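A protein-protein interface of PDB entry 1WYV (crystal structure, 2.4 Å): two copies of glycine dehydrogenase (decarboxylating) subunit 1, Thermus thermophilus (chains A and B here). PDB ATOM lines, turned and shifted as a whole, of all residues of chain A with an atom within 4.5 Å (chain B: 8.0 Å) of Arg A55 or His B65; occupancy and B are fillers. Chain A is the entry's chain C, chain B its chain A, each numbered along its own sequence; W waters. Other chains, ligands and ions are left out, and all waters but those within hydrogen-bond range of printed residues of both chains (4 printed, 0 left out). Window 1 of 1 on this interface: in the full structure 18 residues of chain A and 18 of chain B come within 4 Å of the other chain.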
ATOM      1  N   LEU A  51       8.574  28.689  26.519  1.00  0.00           N
ATOM      2  CA  LEU A  51       8.985  27.299  26.646  1.00  0.00           C
ATOM      3  C   LEU A  51       9.328  26.709  25.284  1.00  0.00           C
ATOM      4  O   LEU A  51      10.252  25.897  25.169  1.00  0.00           O
ATOM      5  CB  LEU A  51       7.881  26.473  27.298  1.00  0.00           C
ATOM      6  CG  LEU A  51       7.704  26.696  28.795  1.00  0.00           C
ATOM      7  CD1 LEU A  51       6.560  25.835  29.297  1.00  0.00           C
ATOM      8  CD2 LEU A  51       8.994  26.350  29.519  1.00  0.00           C
ATOM      9  N   GLU A  52       8.582  27.114  24.258  1.00  0.00           N
ATOM     10  CA  GLU A  52       8.834  26.619  22.908  1.00  0.00           C
ATOM     11  C   GLU A  52      10.232  27.027  22.479  1.00  0.00           C
ATOM     12  O   GLU A  52      10.948  26.247  21.867  1.00  0.00           O
ATOM     13  CB  GLU A  52       7.814  27.177  21.913  1.00  0.00           C
ATOM     14  CG  GLU A  52       7.997  26.647  20.501  1.00  0.00           C
ATOM     15  CD  GLU A  52       6.802  26.920  19.601  1.00  0.00           C
ATOM     16  OE1 GLU A  52       6.679  28.042  19.063  1.00  0.00           O
ATOM     17  OE2 GLU A  52       5.971  26.004  19.438  1.00  0.00           O
ATOM     18  N   GLU A  53      10.614  28.254  22.810  1.00  0.00           N
ATOM     19  CA  GLU A  53      11.935  28.764  22.464  1.00  0.00           C
ATOM     20  C   GLU A  53      13.029  28.058  23.260  1.00  0.00           C
ATOM     21  O   GLU A  53      14.063  27.688  22.703  1.00  0.00           O
ATOM     22  CB  GLU A  53      11.997  30.272  22.696  1.00  0.00           C
ATOM     23  CG  GLU A  53      11.188  31.070  21.681  1.00  0.00           C
ATOM     24  CD  GLU A  53      11.542  30.716  20.242  1.00  0.00           C
ATOM     25  OE1 GLU A  53      12.745  30.757  19.891  1.00  0.00           O
ATOM     26  OE2 GLU A  53      10.615  30.397  19.463  1.00  0.00           O
ATOM     27  N   LEU A  54      12.801  27.871  24.559  1.00  0.00           N
ATOM     28  CA  LEU A  54      13.770  27.170  25.387  1.00  0.00           C
ATOM     29  C   LEU A  54      14.021  25.795  24.761  1.00  0.00           C
ATOM     30  O   LEU A  54      15.169  25.408  24.519  1.00  0.00           O
ATOM     31  CB  LEU A  54      13.239  26.980  26.817  1.00  0.00           C
ATOM     32  CG  LEU A  54      13.512  27.995  27.936  1.00  0.00           C
ATOM     33  CD1 LEU A  54      14.672  28.884  27.557  1.00  0.00           C
ATOM     34  CD2 LEU A  54      12.274  28.816  28.204  1.00  0.00           C
ATOM     35  N   ARG A  55      12.936  25.069  24.493  1.00  0.00           N
ATOM     36  CA  ARG A  55      13.032  23.737  23.906  1.00  0.00           C
ATOM     37  C   ARG A  55      13.741  23.732  22.555  1.00  0.00           C
ATOM     38  O   ARG A  55      14.403  22.760  22.200  1.00  0.00           O
ATOM     39  CB  ARG A  55      11.641  23.101  23.778  1.00  0.00           C
ATOM     40  CG  ARG A  55      11.041  22.690  25.123  1.00  0.00           C
ATOM     41  CD  ARG A  55       9.899  21.687  24.964  1.00  0.00           C
ATOM     42  NE  ARG A  55       8.637  22.321  24.591  1.00  0.00           N
ATOM     43  CZ  ARG A  55       7.820  22.921  25.450  1.00  0.00           C
ATOM     44  NH1 ARG A  55       8.127  22.964  26.738  1.00  0.00           N
ATOM     45  NH2 ARG A  55       6.704  23.488  25.021  1.00  0.00           N
ATOM     46  N   ARG A  56      13.608  24.807  21.793  1.00  0.00           N
ATOM     47  CA  ARG A  56      14.290  24.837  20.514  1.00  0.00           C
ATOM     48  C   ARG A  56      15.790  24.949  20.747  1.00  0.00           C
ATOM     49  O   ARG A  56      16.575  24.296  20.064  1.00  0.00           O
ATOM     50  CB  ARG A  56      13.771  25.988  19.650  1.00  0.00           C
ATOM     51  CG  ARG A  56      12.394  25.676  19.083  1.00  0.00           C
ATOM     52  CD  ARG A  56      11.826  26.786  18.222  1.00  0.00           C
ATOM     53  NE  ARG A  56      10.522  26.396  17.688  1.00  0.00           N
ATOM     54  CZ  ARG A  56       9.780  27.154  16.888  1.00  0.00           C
ATOM     55  NH1 ARG A  56      10.208  28.356  16.520  1.00  0.00           N
ATOM     56  NH2 ARG A  56       8.611  26.704  16.448  1.00  0.00           N
ATOM     57  N   LEU A  57      16.184  25.762  21.724  1.00  0.00           N
ATOM     58  CA  LEU A  57      17.594  25.924  22.046  1.00  0.00           C
ATOM     59  C   LEU A  57      18.123  24.590  22.575  1.00  0.00           C
ATOM     60  O   LEU A  57      19.179  24.115  22.145  1.00  0.00           O
ATOM     61  CB  LEU A  57      17.785  27.013  23.108  1.00  0.00           C
ATOM     62  CG  LEU A  57      17.396  28.450  22.751  1.00  0.00           C
ATOM     63  CD1 LEU A  57      17.543  29.344  23.969  1.00  0.00           C
ATOM     64  CD2 LEU A  57      18.272  28.955  21.628  1.00  0.00           C
ATOM     65  N   ALA A  58      17.377  23.986  23.500  1.00  0.00           N
ATOM     66  CA  ALA A  58      17.765  22.707  24.086  1.00  0.00           C
ATOM     67  C   ALA A  58      17.909  21.632  23.008  1.00  0.00           C
ATOM     68  O   ALA A  58      18.792  20.771  23.083  1.00  0.00           O
ATOM     69  CB  ALA A  58      16.733  22.276  25.111  1.00  0.00           C
ATOM     70  N   ALA A  59      17.037  21.697  22.006  1.00  0.00           N
ATOM     71  CA  ALA A  59      17.044  20.747  20.899  1.00  0.00           C
ATOM     72  C   ALA A  59      18.301  20.903  20.049  1.00  0.00           C
ATOM     73  O   ALA A  59      18.610  20.046  19.221  1.00  0.00           O
ATOM     74  CB  ALA A  59      15.793  20.942  20.027  1.00  0.00           C
ATOM     75  N   LEU B  62       6.625   9.289  19.144  1.00  0.00           N
ATOM     76  CA  LEU B  62       6.753  10.599  18.535  1.00  0.00           C
ATOM     77  C   LEU B  62       5.850  11.452  19.422  1.00  0.00           C
ATOM     78  O   LEU B  62       4.631  11.317  19.375  1.00  0.00           O
ATOM     79  CB  LEU B  62       6.231  10.565  17.094  1.00  0.00           C
ATOM     80  CG  LEU B  62       6.575  11.737  16.165  1.00  0.00           C
ATOM     81  CD1 LEU B  62       5.939  11.499  14.802  1.00  0.00           C
ATOM     82  CD2 LEU B  62       6.069  13.047  16.748  1.00  0.00           C
ATOM     83  N   PRO B  63       6.438  12.321  20.264  1.00  0.00           N
ATOM     84  CA  PRO B  63       5.630  13.164  21.148  1.00  0.00           C
ATOM     85  C   PRO B  63       4.492  13.882  20.430  1.00  0.00           C
ATOM     86  O   PRO B  63       4.615  14.266  19.268  1.00  0.00           O
ATOM     87  CB  PRO B  63       6.661  14.116  21.768  1.00  0.00           C
ATOM     88  CG  PRO B  63       7.752  14.149  20.765  1.00  0.00           C
ATOM     89  CD  PRO B  63       7.853  12.714  20.324  1.00  0.00           C
ATOM     90  N   ALA B  64       3.380  14.055  21.138  1.00  0.00           N
ATOM     91  CA  ALA B  64       2.198  14.687  20.575  1.00  0.00           C
ATOM     92  C   ALA B  64       2.028  16.152  20.953  1.00  0.00           C
ATOM     93  O   ALA B  64       0.938  16.706  20.830  1.00  0.00           O
ATOM     94  CB  ALA B  64       0.960  13.895  20.975  1.00  0.00           C
ATOM     95  N   HIS B  65       3.098  16.780  21.419  1.00  0.00           N
ATOM     96  CA  HIS B  65       3.038  18.192  21.779  1.00  0.00           C
ATOM     97  C   HIS B  65       2.675  18.979  20.512  1.00  0.00           C
ATOM     98  O   HIS B  65       3.319  18.818  19.476  1.00  0.00           O
ATOM     99  CB  HIS B  65       4.395  18.645  22.324  1.00  0.00           C
ATOM    100  CG  HIS B  65       4.447  20.094  22.681  1.00  0.00           C
ATOM    101  ND1 HIS B  65       3.597  20.665  23.605  1.00  0.00           N
ATOM    102  CD2 HIS B  65       5.234  21.097  22.223  1.00  0.00           C
ATOM    103  CE1 HIS B  65       3.856  21.956  23.700  1.00  0.00           C
ATOM    104  NE2 HIS B  65       4.845  22.245  22.871  1.00  0.00           N
ATOM    105  N   LYS B  66       1.637  19.808  20.592  1.00  0.00           N
ATOM    106  CA  LYS B  66       1.175  20.607  19.447  1.00  0.00           C
ATOM    107  C   LYS B  66       0.537  19.801  18.305  1.00  0.00           C
ATOM    108  O   LYS B  66       0.550  20.229  17.149  1.00  0.00           O
ATOM    109  CB  LYS B  66       2.319  21.456  18.877  1.00  0.00           C
ATOM    110  CG  LYS B  66       2.708  22.648  19.740  1.00  0.00           C
ATOM    111  CD  LYS B  66       3.940  23.364  19.184  1.00  0.00           C
ATOM    112  CE  LYS B  66       3.716  23.901  17.774  1.00  0.00           C
ATOM    113  NZ  LYS B  66       4.935  24.584  17.254  1.00  0.00           N
ATOM    114  N   ALA B  67      -0.021  18.640  18.622  1.00  0.00           N
ATOM    115  CA  ALA B  67      -0.673  17.821  17.607  1.00  0.00           C
ATOM    116  C   ALA B  67      -1.972  18.492  17.160  1.00  0.00           C
ATOM    117  O   ALA B  67      -2.521  19.339  17.865  1.00  0.00           O
ATOM    118  CB  ALA B  67      -0.970  16.432  18.160  1.00  0.00           C
ATOM    119  N   PHE B  68      -2.447  18.114  15.979  1.00  0.00           N
ATOM    120  CA  PHE B  68      -3.685  18.661  15.442  1.00  0.00           C
ATOM    121  C   PHE B  68      -4.786  17.615  15.557  1.00  0.00           C
ATOM    122  O   PHE B  68      -5.844  17.724  14.934  1.00  0.00           O
ATOM    123  CB  PHE B  68      -3.487  19.075  13.985  1.00  0.00           C
ATOM    124  CG  PHE B  68      -2.603  20.281  13.817  1.00  0.00           C
ATOM    125  CD1 PHE B  68      -3.095  21.559  14.064  1.00  0.00           C
ATOM    126  CD2 PHE B  68      -1.275  20.138  13.421  1.00  0.00           C
ATOM    127  CE1 PHE B  68      -2.277  22.682  13.917  1.00  0.00           C
ATOM    128  CE2 PHE B  68      -0.444  21.253  13.272  1.00  0.00           C
ATOM    129  CZ  PHE B  68      -0.947  22.526  13.520  1.00  0.00           C
ATOM    130  N   SER B  75      -4.021  19.000  22.465  1.00  0.00           N
ATOM    131  CA  SER B  75      -2.753  19.468  22.999  1.00  0.00           C
ATOM    132  C   SER B  75      -2.803  20.931  23.466  1.00  0.00           C
ATOM    133  O   SER B  75      -2.431  21.844  22.727  1.00  0.00           O
ATOM    134  CB  SER B  75      -1.659  19.288  21.948  1.00  0.00           C
ATOM    135  OG  SER B  75      -0.385  19.517  22.513  1.00  0.00           O
ATOM    136  N   HIS B  76      -3.265  21.140  24.697  1.00  0.00           N
ATOM    137  CA  HIS B  76      -3.349  22.474  25.283  1.00  0.00           C
ATOM    138  C   HIS B  76      -2.106  22.736  26.133  1.00  0.00           C
ATOM    139  O   HIS B  76      -1.333  21.818  26.432  1.00  0.00           O
ATOM    140  CB  HIS B  76      -4.599  22.600  26.160  1.00  0.00           C
ATOM    141  CG  HIS B  76      -5.878  22.712  25.389  1.00  0.00           C
ATOM    142  ND1 HIS B  76      -6.241  23.856  24.709  1.00  0.00           N
ATOM    143  CD2 HIS B  76      -6.870  21.814  25.168  1.00  0.00           C
ATOM    144  CE1 HIS B  76      -7.398  23.657  24.102  1.00  0.00           C
ATOM    145  NE2 HIS B  76      -7.800  22.426  24.363  1.00  0.00           N
ATOM    146  N   HIS B  77      -1.909  23.991  26.522  1.00  0.00           N
ATOM    147  CA  HIS B  77      -0.762  24.341  27.340  1.00  0.00           C
ATOM    148  C   HIS B  77      -0.980  23.848  28.763  1.00  0.00           C
ATOM    149  O   HIS B  77      -2.035  24.077  29.358  1.00  0.00           O
ATOM    150  CB  HIS B  77      -0.545  25.854  27.354  1.00  0.00           C
ATOM    151  CG  HIS B  77       0.517  26.297  28.313  1.00  0.00           C
ATOM    152  ND1 HIS B  77       1.827  25.872  28.223  1.00  0.00           N
ATOM    153  CD2 HIS B  77       0.456  27.106  29.400  1.00  0.00           C
ATOM    154  CE1 HIS B  77       2.525  26.400  29.213  1.00  0.00           C
ATOM    155  NE2 HIS B  77       1.718  27.153  29.942  1.00  0.00           N
ATOM    156  N   VAL B  78       0.016  23.151  29.292  1.00  0.00           N
ATOM    157  CA  VAL B  78      -0.050  22.639  30.652  1.00  0.00           C
ATOM    158  C   VAL B  78       0.824  23.583  31.454  1.00  0.00           C
ATOM    159  O   VAL B  78       2.050  23.471  31.442  1.00  0.00           O
ATOM    160  CB  VAL B  78       0.510  21.209  30.740  1.00  0.00           C
ATOM    161  CG1 VAL B  78       0.468  20.720  32.179  1.00  0.00           C
ATOM    162  CG2 VAL B  78      -0.290  20.286  29.834  1.00  0.00           C
ATOM    163  N   MET B 262      -2.103  15.348  28.275  1.00  0.00           N
ATOM    164  CA  MET B 262      -2.872  14.367  27.519  1.00  0.00           C
ATOM    165  C   MET B 262      -2.634  12.953  28.062  1.00  0.00           C
ATOM    166  O   MET B 262      -3.559  12.142  28.130  1.00  0.00           O
ATOM    167  CB  MET B 262      -2.511  14.448  26.031  1.00  0.00           C
ATOM    168  CG  MET B 262      -2.766  15.822  25.395  1.00  0.00           C
ATOM    169  SD  MET B 262      -2.479  15.861  23.594  1.00  0.00           S
ATOM    170  CE  MET B 262      -0.722  15.980  23.578  1.00  0.00           C
ATOM    171  N   GLY B 397       6.308  13.476  10.370  1.00  0.00           N
ATOM    172  CA  GLY B 397       6.437  14.181  11.632  1.00  0.00           C
ATOM    173  C   GLY B 397       5.246  15.022  12.052  1.00  0.00           C
ATOM    174  O   GLY B 397       5.395  15.928  12.868  1.00  0.00           O
ATOM    175  N   HIS B 399       1.251  15.100  13.642  1.00  0.00           N
ATOM    176  CA  HIS B 399       0.169  14.383  14.300  1.00  0.00           C
ATOM    177  C   HIS B 399      -1.132  15.068  13.908  1.00  0.00           C
ATOM    178  O   HIS B 399      -1.418  16.179  14.356  1.00  0.00           O
ATOM    179  CB  HIS B 399       0.327  14.422  15.819  1.00  0.00           C
ATOM    180  CG  HIS B 399       1.363  13.479  16.345  1.00  0.00           C
ATOM    181  ND1 HIS B 399       1.348  12.128  16.068  1.00  0.00           N
ATOM    182  CD2 HIS B 399       2.420  13.683  17.167  1.00  0.00           C
ATOM    183  CE1 HIS B 399       2.350  11.539  16.698  1.00  0.00           C
ATOM    184  NE2 HIS B 399       3.015  12.461  17.371  1.00  0.00           N
ATOM    185  N   THR B 418      -5.334  24.562  19.019  1.00  0.00           N
ATOM    186  CA  THR B 418      -5.328  25.065  20.382  1.00  0.00           C
ATOM    187  C   THR B 418      -4.583  26.390  20.457  1.00  0.00           C
ATOM    188  O   THR B 418      -4.060  26.874  19.451  1.00  0.00           O
ATOM    189  CB  THR B 418      -4.663  24.050  21.343  1.00  0.00           C
ATOM    190  OG1 THR B 418      -3.252  24.003  21.098  1.00  0.00           O
ATOM    191  CG2 THR B 418      -5.239  22.660  21.124  1.00  0.00           C
ATOM    192  N   LEU B 420      -1.756  27.047  21.534  1.00  0.00           N
ATOM    193  CA  LEU B 420      -0.309  27.023  21.331  1.00  0.00           C
ATOM    194  C   LEU B 420       0.071  26.818  19.867  1.00  0.00           C
ATOM    195  O   LEU B 420       1.246  26.685  19.526  1.00  0.00           O
ATOM    196  CB  LEU B 420       0.356  25.975  22.233  1.00  0.00           C
ATOM    197  CG  LEU B 420      -0.231  24.577  22.325  1.00  0.00           C
ATOM    198  CD1 LEU B 420      -0.198  23.925  20.954  1.00  0.00           C
ATOM    199  CD2 LEU B 420       0.555  23.767  23.340  1.00  0.00           C
ATOM    200  N   HIS B 421      -0.938  26.810  19.006  1.00  0.00           N
ATOM    201  CA  HIS B 421      -0.734  26.664  17.573  1.00  0.00           C
ATOM    202  C   HIS B 421      -0.612  28.050  16.951  1.00  0.00           C
ATOM    203  O   HIS B 421      -1.440  28.924  17.202  1.00  0.00           O
ATOM    204  CB  HIS B 421      -1.917  25.938  16.944  1.00  0.00           C
ATOM    205  CG  HIS B 421      -1.872  24.454  17.117  1.00  0.00           C
ATOM    206  ND1 HIS B 421      -2.982  23.711  17.459  1.00  0.00           N
ATOM    207  CD2 HIS B 421      -0.861  23.568  16.951  1.00  0.00           C
ATOM    208  CE1 HIS B 421      -2.656  22.432  17.493  1.00  0.00           C
ATOM    209  NE2 HIS B 421      -1.375  22.318  17.188  1.00  0.00           N
HETATM  210  O   HOH W   1       5.269  27.202  15.884  1.00  0.00           O
HETATM  211  O   HOH W   2       4.949  25.122  24.400  1.00  0.00           O
HETATM  212  O   HOH W   3       3.634  24.168  26.534  1.00  0.00           O
HETATM  213  O   HOH W   4       3.462  26.757  18.003  1.00  0.00           O
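The side-chain carboxylate (OE1) of Glu A52 lies within salt-bridge range of the guanidinium group (NH2) of Arg A56 (3.5 Å). A ring nitrogen (NE2) of His B421 lies within hydrogen-bond range of the backbone carbonyl oxygen (O) of Lys B66. The backbone NH of Lys B66 lies within hydrogen-bond range of the side-chain hydroxyl of Ser B75, 2.8 Å away.
Water W2 lies within hydrogen-bond range of the guanidinium group of Arg A55 (2.5 Å) and a ring nitrogen (NE2) of His B65 (3.3 Å). Water W4 lies within hydrogen-bond range of O of Leu B420 (2.7 Å), NZ of Lys B66 (2.7 Å) and OE2 of Glu A52 (3.0 Å). Water W1 lies within hydrogen-bond range of NZ of Lys B66 (3.0 Å) and NH2 of Arg A56 (3.4 Å). Water W3 lies within hydrogen-bond range of a ring nitrogen (ND1) of His B77 and the guanidinium group of Arg A55.
Of the 17 printed residues of chain B, 2 touch a printed residue of chain A. Among the printed residues, 2 pairs touch across the chains. Among the printed residues, Asp or Glu carboxylates within 4 Å of a Lys or Arg side-chain nitrogen of the other chain: Glu A52 with Lys B66 (2.8 Å).
Arg A55 touches just one residue of chain B: His B65. Of the printed residues of chain B, Glu A52 touches Lys B66. Printed residues of chain A within 4 Å of Lys B66: Glu A52 (2.8 Å). The nearest residue of chain B that does not touch Arg A55 is His B77 (6.3 Å). The nearest printed residue of chain A that does not touch His B65 is Glu A52 (5.2 Å). The nearest printed residue of chain B that does not touch Glu A52 is Leu B420 (4.8 Å).
The side-chain amino group (NZ) of Lys B66 lies within salt-bridge range of the side-chain carboxylate (OE2) of Glu A52 (2.8 Å). A ring nitrogen (NE2) of His B65 is in hydrogen-bond range of the guanidinium group (NH2) of Arg A55 (3.1 Å).
No position is printed for both chains. Of the 2 pairs that touch across the chains among the printed residues, none has its exchanged pair printed and touching as well.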
